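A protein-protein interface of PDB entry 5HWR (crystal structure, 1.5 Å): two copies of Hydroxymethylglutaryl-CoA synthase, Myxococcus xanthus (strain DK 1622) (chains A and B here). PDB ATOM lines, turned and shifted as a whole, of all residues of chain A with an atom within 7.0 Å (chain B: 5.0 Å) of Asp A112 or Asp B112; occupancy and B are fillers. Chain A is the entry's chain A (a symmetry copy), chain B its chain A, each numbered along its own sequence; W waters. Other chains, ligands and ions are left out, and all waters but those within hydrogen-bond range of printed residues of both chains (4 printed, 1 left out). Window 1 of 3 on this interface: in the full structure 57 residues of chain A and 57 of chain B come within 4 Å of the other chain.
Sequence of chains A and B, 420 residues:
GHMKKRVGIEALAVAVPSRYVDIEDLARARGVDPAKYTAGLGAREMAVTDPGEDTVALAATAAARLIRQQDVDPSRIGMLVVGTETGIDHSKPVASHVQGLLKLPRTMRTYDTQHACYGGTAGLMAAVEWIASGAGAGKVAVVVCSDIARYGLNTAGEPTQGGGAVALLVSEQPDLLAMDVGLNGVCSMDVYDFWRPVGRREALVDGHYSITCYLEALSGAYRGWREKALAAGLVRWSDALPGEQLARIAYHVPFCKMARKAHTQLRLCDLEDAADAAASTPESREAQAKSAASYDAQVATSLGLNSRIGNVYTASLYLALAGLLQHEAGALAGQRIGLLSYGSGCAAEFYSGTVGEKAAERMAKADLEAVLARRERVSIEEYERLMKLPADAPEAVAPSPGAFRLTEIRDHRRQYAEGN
O of Thr B110 lies within hydrogen-bond range of ND1 of His A115 (2.8 Å). O of Asp B112 lies within hydrogen-bond range of N of Gln A114 (2.9 Å). OE1 of Gln B114 lies close to O of Asp A89 (3.0 Å). O of Ser A91 sits close to OE1 of Gln B114. OE1 of Gln B114 lies close to O of Lys A92. The backbone NH (N) of Gln B114 lies within hydrogen-bond range of the backbone carbonyl oxygen (O) of Asp A112 (2.9 Å).
O of Val B82 lies within hydrogen-bond range of N of Thr B113, at 2.9 Å. The backbone NH (N) of Val A82 is in hydrogen-bond range of the backbone carbonyl oxygen (O) of Tyr A111 (3.1 Å). The backbone carbonyl oxygen (O) of Val A82 lies within hydrogen-bond range of the backbone NH (N) of Thr A113 (2.9 Å). The backbone carbonyl oxygen of Thr A113 is in hydrogen-bond range of the backbone NH of Thr A84 (3.2 Å). OD2 of Asp A89 sits at hydrogen-bond distance from N of Ser A91 (2.9 Å). The side-chain hydroxyl (OG1) of Thr A113 sits at hydrogen-bond distance from the backbone carbonyl oxygen (O) of Gly A119 (2.8 Å).
Pro A93 touches Gln B114 (CB to O, 3.5 Å). Tyr A111 touches Gln B114 (CB to O, 3.4 Å). Asp A112 touches Asp B112 (O to O, 3.98 Å). Asp A112 touches Thr B113. Thr A113 touches Asp B112 (CA to O, 3.4 Å). CB of Pro B93 touches O of Gln A114 (3.5 Å). O of Gln A114 touches CB of Tyr B111, at 3.4 Å. His A115 touches Pro B93. Tyr B111 touches His A115. CB of Ala A122 touches CD1 of Tyr B111, 3.5 Å away.
Of the printed residues of chain B, Asp A112 touches Asp B112 (3.98 Å), Thr B113 (3.4 Å) and Gln B114 (2.9 Å). Printed residues of chain A within 4 Å of Asp B112: Asp A112, Thr A113 and Gln A114. Of the printed residues of chain B, Gln A114 touches Pro B93, Tyr B111 and Asp B112. Of the printed residues of chain B, Ser A91 touches Gln B114. Of the printed residues of chain B, Lys A92 touches Gln B114. Of the printed residues of chain B, Asp A89 touches Gln B114 (3.0 Å). Printed residues of chain A within 4 Å of Gln B114: Asp A89 (3.0 Å), Ser A91 (3.3 Å), Lys A92 (3.4 Å), Pro A93 (3.5 Å), Tyr A111 (3.4 Å) and Asp A112 (2.9 Å). The nearest printed residue of chain B that does not touch Asp A112 is Tyr B111 (6.3 Å). The nearest printed residue of chain A that does not touch Asp B112 is His A115 (5.1 Å).
Printed residues of chain A that touch a printed residue of chain B: Asp A89, Ser A91, Lys A92, Pro A93, Tyr A111, Asp A112, Thr A113, Gln A114, His A115 and Ala A122. Hydrophobic or aromatic side chains of chain A that line the printed part of chain B: Pro A93, Tyr A111, His A115 and Ala A122. Hydrophobic or aromatic side chains of chain B that line the printed part of chain A: Pro B93 and Tyr B111. Along chain B the printed residues that touch a printed residue of chain A span positions 93 to 114. Among the printed residues, no Asp or Glu carboxylate lies within 4 Å of a Lys or Arg side-chain nitrogen of the other chain.
Pro A93 touches Gln B114, and with the chains exchanged Gln A114 touches Pro B93. Asp B112 touches its own counterpart, Asp A112. Asp A112 touches Thr B113, and with the chains exchanged Thr A113 touches Asp B112. Asp A112 touches Gln B114, and with the chains exchanged Gln A114 touches Asp B112. Of the 16 pairs that touch across the chains among the printed residues, 9 have their exchanged pair printed and touching as well.
Water W1 bridges the side-chain carboxylate (OD2) of Asp B112 (2.6 Å) and the side-chain amide nitrogen (NE2) of Gln A114 (3.2 Å). Water W3 lies within hydrogen-bond range of the side-chain carboxylate (OD2) of Asp A112 and the side-chain amide nitrogen (NE2) of Gln B114. Water W2 bridges OH of Tyr B111 (2.7 Å) and O of Ala A122 (3.1 Å). Water W4 bridges NE2 of Gln B114 (2.8 Å) and NE2 of Gln A114 (2.8 Å).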
ATOM      1  N   THR A  55     -35.684  21.722 -18.551  1.00  0.00           N
ATOM      2  CA  THR A  55     -34.421  21.072 -18.865  1.00  0.00           C
ATOM      3  C   THR A  55     -33.283  22.073 -18.916  1.00  0.00           C
ATOM      4  O   THR A  55     -32.176  21.789 -18.433  1.00  0.00           O
ATOM      5  CB  THR A  55     -34.578  20.341 -20.189  1.00  0.00           C
ATOM      6  OG1 THR A  55     -35.789  19.574 -20.134  1.00  0.00           O
ATOM      7  CG2 THR A  55     -33.385  19.473 -20.466  1.00  0.00           C
ATOM      8  N   LEU A  80     -19.717  22.032 -25.670  1.00  0.00           N
ATOM      9  CA  LEU A  80     -20.789  22.048 -24.673  1.00  0.00           C
ATOM     10  C   LEU A  80     -21.898  21.189 -25.258  1.00  0.00           C
ATOM     11  O   LEU A  80     -22.526  21.578 -26.251  1.00  0.00           O
ATOM     12  CB  LEU A  80     -21.283  23.474 -24.385  1.00  0.00           C
ATOM     13  CG  LEU A  80     -22.499  23.616 -23.453  1.00  0.00           C
ATOM     14  CD1 LEU A  80     -22.185  23.105 -22.057  1.00  0.00           C
ATOM     15  CD2 LEU A  80     -22.969  25.039 -23.390  1.00  0.00           C
ATOM     16  N   VAL A  81     -22.119  20.021 -24.654  1.00  0.00           N
ATOM     17  CA  VAL A  81     -23.100  19.055 -25.133  1.00  0.00           C
ATOM     18  C   VAL A  81     -24.082  18.773 -23.998  1.00  0.00           C
ATOM     19  O   VAL A  81     -23.678  18.597 -22.842  1.00  0.00           O
ATOM     20  CB  VAL A  81     -22.429  17.751 -25.601  1.00  0.00           C
ATOM     21  CG1 VAL A  81     -23.431  16.714 -25.984  1.00  0.00           C
ATOM     22  CG2 VAL A  81     -21.517  18.034 -26.767  1.00  0.00           C
ATOM     23  N   VAL A  82     -25.377  18.754 -24.322  1.00  0.00           N
ATOM     24  CA  VAL A  82     -26.421  18.374 -23.370  1.00  0.00           C
ATOM     25  C   VAL A  82     -27.029  17.067 -23.842  1.00  0.00           C
ATOM     26  O   VAL A  82     -27.596  16.984 -24.943  1.00  0.00           O
ATOM     27  CB  VAL A  82     -27.494  19.453 -23.206  1.00  0.00           C
ATOM     28  CG1 VAL A  82     -28.591  18.976 -22.232  1.00  0.00           C
ATOM     29  CG2 VAL A  82     -26.875  20.762 -22.671  1.00  0.00           C
ATOM     30  N   GLY A  83     -26.892  16.033 -23.011  1.00  0.00           N
ATOM     31  CA  GLY A  83     -27.623  14.799 -23.223  1.00  0.00           C
ATOM     32  C   GLY A  83     -28.961  14.920 -22.516  1.00  0.00           C
ATOM     33  O   GLY A  83     -29.013  15.241 -21.330  1.00  0.00           O
ATOM     34  N   THR A  84     -30.038  14.699 -23.256  1.00  0.00           N
ATOM     35  CA  THR A  84     -31.375  14.826 -22.702  1.00  0.00           C
ATOM     36  C   THR A  84     -32.360  14.043 -23.548  1.00  0.00           C
ATOM     37  O   THR A  84     -32.149  13.844 -24.743  1.00  0.00           O
ATOM     38  CB  THR A  84     -31.792  16.302 -22.608  1.00  0.00           C
ATOM     39  OG1 THR A  84     -33.029  16.438 -21.918  1.00  0.00           O
ATOM     40  CG2 THR A  84     -31.933  16.948 -23.982  1.00  0.00           C
ATOM     41  N   GLY A  87     -36.099  17.354 -24.347  1.00  0.00           N
ATOM     42  CA  GLY A  87     -35.825  18.528 -25.174  1.00  0.00           C
ATOM     43  C   GLY A  87     -37.001  19.491 -25.182  1.00  0.00           C
ATOM     44  O   GLY A  87     -38.162  19.099 -25.042  1.00  0.00           O
ATOM     45  N   ILE A  88     -36.699  20.771 -25.403  1.00  0.00           N
ATOM     46  CA  ILE A  88     -37.740  21.794 -25.372  1.00  0.00           C
ATOM     47  C   ILE A  88     -37.892  22.524 -26.696  1.00  0.00           C
ATOM     48  O   ILE A  88     -38.735  23.425 -26.806  1.00  0.00           O
ATOM     49  CB  ILE A  88     -37.553  22.797 -24.217  1.00  0.00           C
ATOM     50  CG1 ILE A  88     -36.152  23.376 -24.130  1.00  0.00           C
ATOM     51  CG2 ILE A  88     -37.837  22.116 -22.904  1.00  0.00           C
ATOM     52  CD1 ILE A  88     -35.717  24.281 -25.271  1.00  0.00           C
ATOM     53  N   ASP A  89     -37.155  22.118 -27.718  1.00  0.00           N
ATOM     54  CA  ASP A  89     -37.325  22.637 -29.070  1.00  0.00           C
ATOM     55  C   ASP A  89     -36.881  21.537 -30.025  1.00  0.00           C
ATOM     56  O   ASP A  89     -35.950  20.792 -29.715  1.00  0.00           O
ATOM     57  CB  ASP A  89     -36.495  23.915 -29.270  1.00  0.00           C
ATOM     58  CG  ASP A  89     -36.973  24.755 -30.447  1.00  0.00           C
ATOM     59  OD1 ASP A  89     -37.863  25.612 -30.244  1.00  0.00           O
ATOM     60  OD2 ASP A  89     -36.444  24.588 -31.556  1.00  0.00           O
ATOM     61  N   SER A  91     -35.422  22.169 -32.811  1.00  0.00           N
ATOM     62  CA  SER A  91     -34.279  22.724 -33.525  1.00  0.00           C
ATOM     63  C   SER A  91     -33.216  23.300 -32.607  1.00  0.00           C
ATOM     64  O   SER A  91     -32.036  22.932 -32.698  1.00  0.00           O
ATOM     65  CB  SER A  91     -34.781  23.823 -34.441  1.00  0.00           C
ATOM     66  OG  SER A  91     -33.730  24.339 -35.231  1.00  0.00           O
ATOM     67  N   LYS A  92     -33.629  24.184 -31.733  1.00  0.00           N
ATOM     68  CA  LYS A  92     -32.707  24.927 -30.896  1.00  0.00           C
ATOM     69  C   LYS A  92     -32.320  24.041 -29.720  1.00  0.00           C
ATOM     70  O   LYS A  92     -33.206  23.617 -28.966  1.00  0.00           O
ATOM     71  CB  LYS A  92     -33.353  26.222 -30.406  1.00  0.00           C
ATOM     72  CG  LYS A  92     -32.416  27.097 -29.586  1.00  0.00           C
ATOM     73  CD  LYS A  92     -33.035  28.468 -29.328  1.00  0.00           C
ATOM     74  CE  LYS A  92     -32.233  29.291 -28.343  1.00  0.00           C
ATOM     75  NZ  LYS A  92     -30.868  29.545 -28.808  1.00  0.00           N
ATOM     76  N   PRO A  93     -31.043  23.732 -29.532  1.00  0.00           N
ATOM     77  CA  PRO A  93     -30.682  22.744 -28.513  1.00  0.00           C
ATOM     78  C   PRO A  93     -30.615  23.375 -27.131  1.00  0.00           C
ATOM     79  O   PRO A  93     -30.342  24.573 -26.978  1.00  0.00           O
ATOM     80  CB  PRO A  93     -29.299  22.260 -28.968  1.00  0.00           C
ATOM     81  CG  PRO A  93     -28.713  23.478 -29.681  1.00  0.00           C
ATOM     82  CD  PRO A  93     -29.881  24.135 -30.351  1.00  0.00           C
ATOM     83  N   VAL A  94     -30.851  22.544 -26.123  1.00  0.00           N
ATOM     84  CA  VAL A  94     -30.647  22.977 -24.740  1.00  0.00           C
ATOM     85  C   VAL A  94     -29.249  23.567 -24.574  1.00  0.00           C
ATOM     86  O   VAL A  94     -29.057  24.578 -23.879  1.00  0.00           O
ATOM     87  CB  VAL A  94     -30.902  21.803 -23.778  1.00  0.00           C
ATOM     88  CG1 VAL A  94     -30.625  22.208 -22.369  1.00  0.00           C
ATOM     89  CG2 VAL A  94     -32.349  21.331 -23.887  1.00  0.00           C
ATOM     90  N   ALA A  95     -28.254  22.965 -25.227  1.00  0.00           N
ATOM     91  CA  ALA A  95     -26.881  23.451 -25.112  1.00  0.00           C
ATOM     92  C   ALA A  95     -26.743  24.921 -25.511  1.00  0.00           C
ATOM     93  O   ALA A  95     -25.941  25.644 -24.927  1.00  0.00           O
ATOM     94  CB  ALA A  95     -25.952  22.621 -25.970  1.00  0.00           C
ATOM     95  N   SER A  96     -27.482  25.375 -26.521  1.00  0.00           N
ATOM     96  CA  SER A  96     -27.388  26.793 -26.907  1.00  0.00           C
ATOM     97  C   SER A  96     -27.978  27.710 -25.853  1.00  0.00           C
ATOM     98  O   SER A  96     -27.427  28.787 -25.590  1.00  0.00           O
ATOM     99  CB  SER A  96     -28.040  27.052 -28.272  1.00  0.00           C
ATOM    100  OG  SER A  96     -29.445  26.959 -28.279  1.00  0.00           O
ATOM    101  N   THR A 110     -21.658  23.445 -29.876  1.00  0.00           N
ATOM    102  CA  THR A 110     -22.821  23.252 -29.017  1.00  0.00           C
ATOM    103  C   THR A 110     -23.810  22.329 -29.722  1.00  0.00           C
ATOM    104  O   THR A 110     -24.093  22.506 -30.910  1.00  0.00           O
ATOM    105  CB  THR A 110     -23.505  24.562 -28.653  1.00  0.00           C
ATOM    106  OG1 THR A 110     -23.998  25.216 -29.816  1.00  0.00           O
ATOM    107  CG2 THR A 110     -22.576  25.499 -27.944  1.00  0.00           C
ATOM    108  N   TYR A 111     -24.331  21.342 -28.994  1.00  0.00           N
ATOM    109  CA  TYR A 111     -25.402  20.493 -29.514  1.00  0.00           C
ATOM    110  C   TYR A 111     -25.936  19.641 -28.378  1.00  0.00           C
ATOM    111  O   TYR A 111     -25.326  19.535 -27.314  1.00  0.00           O
ATOM    112  CB  TYR A 111     -24.955  19.641 -30.700  1.00  0.00           C
ATOM    113  CG  TYR A 111     -23.794  18.686 -30.489  1.00  0.00           C
ATOM    114  CD1 TYR A 111     -22.482  19.090 -30.682  1.00  0.00           C
ATOM    115  CD2 TYR A 111     -24.015  17.348 -30.162  1.00  0.00           C
ATOM    116  CE1 TYR A 111     -21.436  18.180 -30.532  1.00  0.00           C
ATOM    117  CE2 TYR A 111     -22.984  16.475 -30.030  1.00  0.00           C
ATOM    118  CZ  TYR A 111     -21.697  16.879 -30.223  1.00  0.00           C
ATOM    119  OH  TYR A 111     -20.687  15.944 -30.102  1.00  0.00           O
ATOM    120  N   ASP A 112     -27.082  19.031 -28.637  1.00  0.00           N
ATOM    121  CA  ASP A 112     -27.667  18.034 -27.761  1.00  0.00           C
ATOM    122  C   ASP A 112     -27.526  16.641 -28.365  1.00  0.00           C
ATOM    123  O   ASP A 112     -27.532  16.460 -29.586  1.00  0.00           O
ATOM    124  CB  ASP A 112     -29.148  18.316 -27.495  1.00  0.00           C
ATOM    125  CG  ASP A 112     -29.433  19.631 -26.776  1.00  0.00           C
ATOM    126  OD1 ASP A 112     -28.516  20.341 -26.313  1.00  0.00           O
ATOM    127  OD2 ASP A 112     -30.673  19.930 -26.675  1.00  0.00           O
ATOM    128  N   THR A 113     -27.440  15.656 -27.479  1.00  0.00           N
ATOM    129  CA  THR A 113     -27.432  14.247 -27.881  1.00  0.00           C
ATOM    130  C   THR A 113     -28.653  13.545 -27.318  1.00  0.00           C
ATOM    131  O   THR A 113     -29.051  13.799 -26.181  1.00  0.00           O
ATOM    132  CB  THR A 113     -26.169  13.552 -27.408  1.00  0.00           C
ATOM    133  OG1 THR A 113     -25.918  13.895 -26.046  1.00  0.00           O
ATOM    134  CG2 THR A 113     -24.985  13.979 -28.242  1.00  0.00           C
ATOM    135  N   GLN A 114     -29.246  12.657 -28.127  1.00  0.00           N
ATOM    136  CA  GLN A 114     -30.512  12.012 -27.784  1.00  0.00           C
ATOM    137  C   GLN A 114     -30.436  10.508 -28.015  1.00  0.00           C
ATOM    138  O   GLN A 114     -30.299  10.050 -29.151  1.00  0.00           O
ATOM    139  CB  GLN A 114     -31.695  12.563 -28.595  1.00  0.00           C
ATOM    140  CG  GLN A 114     -33.038  11.904 -28.104  1.00  0.00           C
ATOM    141  CD  GLN A 114     -34.223  12.122 -29.016  1.00  0.00           C
ATOM    142  OE1 GLN A 114     -34.999  11.195 -29.325  1.00  0.00           O
ATOM    143  NE2 GLN A 114     -34.400  13.345 -29.410  1.00  0.00           N
ATOM    144  N   HIS A 115     -30.597   9.760 -26.940  1.00  0.00           N
ATOM    145  CA  HIS A 115     -31.028   8.373 -26.993  1.00  0.00           C
ATOM    146  C   HIS A 115     -31.487   8.015 -25.595  1.00  0.00           C
ATOM    147  O   HIS A 115     -30.717   7.429 -24.830  1.00  0.00           O
ATOM    148  CB  HIS A 115     -29.955   7.403 -27.475  1.00  0.00           C
ATOM    149  CG  HIS A 115     -30.491   6.017 -27.654  1.00  0.00           C
ATOM    150  ND1 HIS A 115     -29.923   5.083 -28.491  1.00  0.00           N
ATOM    151  CD2 HIS A 115     -31.629   5.454 -27.188  1.00  0.00           C
ATOM    152  CE1 HIS A 115     -30.658   3.985 -28.487  1.00  0.00           C
ATOM    153  NE2 HIS A 115     -31.702   4.187 -27.715  1.00  0.00           N
ATOM    154  N   GLY A 119     -28.222   9.215 -23.733  1.00  0.00           N
ATOM    155  CA  GLY A 119     -27.746  10.407 -24.425  1.00  0.00           C
ATOM    156  C   GLY A 119     -26.572  11.104 -23.754  1.00  0.00           C
ATOM    157  O   GLY A 119     -25.719  11.670 -24.434  1.00  0.00           O
ATOM    158  N   ALA A 122     -23.418   9.155 -24.592  1.00  0.00           N
ATOM    159  CA  ALA A 122     -23.054   9.412 -25.981  1.00  0.00           C
ATOM    160  C   ALA A 122     -22.272  10.708 -26.119  1.00  0.00           C
ATOM    161  O   ALA A 122     -21.259  10.761 -26.823  1.00  0.00           O
ATOM    162  CB  ALA A 122     -24.297   9.469 -26.843  1.00  0.00           C
ATOM    163  N   VAL B  81     -25.262   7.430 -36.156  1.00  0.00           N
ATOM    164  CA  VAL B  81     -25.730   8.700 -35.613  1.00  0.00           C
ATOM    165  C   VAL B  81     -26.608   9.371 -36.666  1.00  0.00           C
ATOM    166  O   VAL B  81     -26.267   9.392 -37.854  1.00  0.00           O
ATOM    167  CB  VAL B  81     -24.556   9.618 -35.225  1.00  0.00           C
ATOM    168  CG1 VAL B  81     -25.023  10.962 -34.778  1.00  0.00           C
ATOM    169  CG2 VAL B  81     -23.740   8.973 -34.136  1.00  0.00           C
ATOM    170  N   VAL B  82     -27.756   9.902 -36.234  1.00  0.00           N
ATOM    171  CA  VAL B  82     -28.636  10.685 -37.101  1.00  0.00           C
ATOM    172  C   VAL B  82     -28.628  12.118 -36.603  1.00  0.00           C
ATOM    173  O   VAL B  82     -29.020  12.401 -35.459  1.00  0.00           O
ATOM    174  CB  VAL B  82     -30.061  10.129 -37.155  1.00  0.00           C
ATOM    175  CG1 VAL B  82     -30.953  11.022 -38.041  1.00  0.00           C
ATOM    176  CG2 VAL B  82     -30.066   8.692 -37.717  1.00  0.00           C
ATOM    177  N   THR B  84     -30.474  15.502 -36.974  1.00  0.00           N
ATOM    178  CA  THR B  84     -31.792  15.931 -37.412  1.00  0.00           C
ATOM    179  C   THR B  84     -32.306  17.027 -36.499  1.00  0.00           C
ATOM    180  O   THR B  84     -31.933  17.105 -35.330  1.00  0.00           O
ATOM    181  CB  THR B  84     -32.772  14.747 -37.444  1.00  0.00           C
ATOM    182  OG1 THR B  84     -34.013  15.131 -38.024  1.00  0.00           O
ATOM    183  CG2 THR B  84     -33.043  14.187 -36.052  1.00  0.00           C
ATOM    184  N   PRO B  93     -34.479   7.518 -30.477  1.00  0.00           N
ATOM    185  CA  PRO B  93     -33.841   8.296 -31.540  1.00  0.00           C
ATOM    186  C   PRO B  93     -34.148   7.716 -32.913  1.00  0.00           C
ATOM    187  O   PRO B  93     -34.392   6.512 -33.066  1.00  0.00           O
ATOM    188  CB  PRO B  93     -32.347   8.178 -31.212  1.00  0.00           C
ATOM    189  CG  PRO B  93     -32.239   6.815 -30.530  1.00  0.00           C
ATOM    190  CD  PRO B  93     -33.512   6.669 -29.753  1.00  0.00           C
ATOM    191  N   VAL B  94     -34.116   8.589 -33.911  1.00  0.00           N
ATOM    192  CA  VAL B  94     -34.220   8.136 -35.299  1.00  0.00           C
ATOM    193  C   VAL B  94     -33.195   7.038 -35.572  1.00  0.00           C
ATOM    194  O   VAL B  94     -33.483   6.048 -36.262  1.00  0.00           O
ATOM    195  CB  VAL B  94     -34.063   9.330 -36.257  1.00  0.00           C
ATOM    196  CG1 VAL B  94     -34.092   8.874 -37.677  1.00  0.00           C
ATOM    197  CG2 VAL B  94     -35.186  10.340 -36.034  1.00  0.00           C
ATOM    198  N   ALA B  95     -31.990   7.180 -35.015  1.00  0.00           N
ATOM    199  CA  ALA B  95     -30.942   6.187 -35.237  1.00  0.00           C
ATOM    200  C   ALA B  95     -31.371   4.778 -34.825  1.00  0.00           C
ATOM    201  O   ALA B  95     -30.978   3.804 -35.462  1.00  0.00           O
ATOM    202  CB  ALA B  95     -29.690   6.560 -34.475  1.00  0.00           C
ATOM    203  N   THR B 110     -25.772   4.017 -30.931  1.00  0.00           N
ATOM    204  CA  THR B 110     -26.829   4.674 -31.693  1.00  0.00           C
ATOM    205  C   THR B 110     -27.302   5.903 -30.923  1.00  0.00           C
ATOM    206  O   THR B 110     -27.532   5.834 -29.713  1.00  0.00           O
ATOM    207  CB  THR B 110     -28.008   3.755 -31.974  1.00  0.00           C
ATOM    208  OG1 THR B 110     -28.622   3.333 -30.763  1.00  0.00           O
ATOM    209  CG2 THR B 110     -27.596   2.537 -32.743  1.00  0.00           C
ATOM    210  N   TYR B 111     -27.444   7.030 -31.622  1.00  0.00           N
ATOM    211  CA  TYR B 111     -28.037   8.228 -31.028  1.00  0.00           C
ATOM    212  C   TYR B 111     -28.279   9.241 -32.130  1.00  0.00           C
ATOM    213  O   TYR B 111     -27.770   9.113 -33.244  1.00  0.00           O
ATOM    214  CB  TYR B 111     -27.188   8.808 -29.899  1.00  0.00           C
ATOM    215  CG  TYR B 111     -25.764   9.221 -30.225  1.00  0.00           C
ATOM    216  CD1 TYR B 111     -24.713   8.323 -30.136  1.00  0.00           C
ATOM    217  CD2 TYR B 111     -25.457  10.542 -30.555  1.00  0.00           C
ATOM    218  CE1 TYR B 111     -23.406   8.740 -30.389  1.00  0.00           C
ATOM    219  CE2 TYR B 111     -24.178  10.931 -30.789  1.00  0.00           C
ATOM    220  CZ  TYR B 111     -23.149  10.042 -30.699  1.00  0.00           C
ATOM    221  OH  TYR B 111     -21.863  10.496 -30.920  1.00  0.00           O
ATOM    222  N   ASP B 112     -29.059  10.254 -31.786  1.00  0.00           N
ATOM    223  CA  ASP B 112     -29.267  11.418 -32.627  1.00  0.00           C
ATOM    224  C   ASP B 112     -28.529  12.627 -32.063  1.00  0.00           C
ATOM    225  O   ASP B 112     -28.360  12.774 -30.848  1.00  0.00           O
ATOM    226  CB  ASP B 112     -30.753  11.758 -32.763  1.00  0.00           C
ATOM    227  CG  ASP B 112     -31.601  10.679 -33.432  1.00  0.00           C
ATOM    228  OD1 ASP B 112     -31.088   9.670 -33.957  1.00  0.00           O
ATOM    229  OD2 ASP B 112     -32.860  10.903 -33.423  1.00  0.00           O
ATOM    230  N   THR B 113     -28.131  13.511 -32.970  1.00  0.00           N
ATOM    231  CA  THR B 113     -27.526  14.791 -32.594  1.00  0.00           C
ATOM    232  C   THR B 113     -28.406  15.934 -33.065  1.00  0.00           C
ATOM    233  O   THR B 113     -28.967  15.879 -34.159  1.00  0.00           O
ATOM    234  CB  THR B 113     -26.135  14.930 -33.184  1.00  0.00           C
ATOM    235  OG1 THR B 113     -26.158  14.540 -34.557  1.00  0.00           O
ATOM    236  CG2 THR B 113     -25.155  14.050 -32.446  1.00  0.00           C
ATOM    237  N   GLN B 114     -28.524  16.970 -32.225  1.00  0.00           N
ATOM    238  CA  GLN B 114     -29.450  18.074 -32.470  1.00  0.00           C
ATOM    239  C   GLN B 114     -28.758  19.416 -32.274  1.00  0.00           C
ATOM    240  O   GLN B 114     -28.354  19.762 -31.162  1.00  0.00           O
ATOM    241  CB  GLN B 114     -30.681  18.028 -31.554  1.00  0.00           C
ATOM    242  CG  GLN B 114     -31.684  19.179 -31.941  1.00  0.00           C
ATOM    243  CD  GLN B 114     -32.776  19.438 -30.929  1.00  0.00           C
ATOM    244  OE1 GLN B 114     -33.087  20.592 -30.572  1.00  0.00           O
ATOM    245  NE2 GLN B 114     -33.393  18.380 -30.500  1.00  0.00           N
HETATM  246  O   HOH W   1     -34.436  12.844 -32.606  1.00  0.00           O
HETATM  247  O   HOH W   2     -20.056   9.347 -29.307  1.00  0.00           O
HETATM  248  O   HOH W   3     -32.956  18.798 -27.322  1.00  0.00           O
HETATM  249  O   HOH W   4     -33.037  15.683 -29.993  1.00  0.00           O
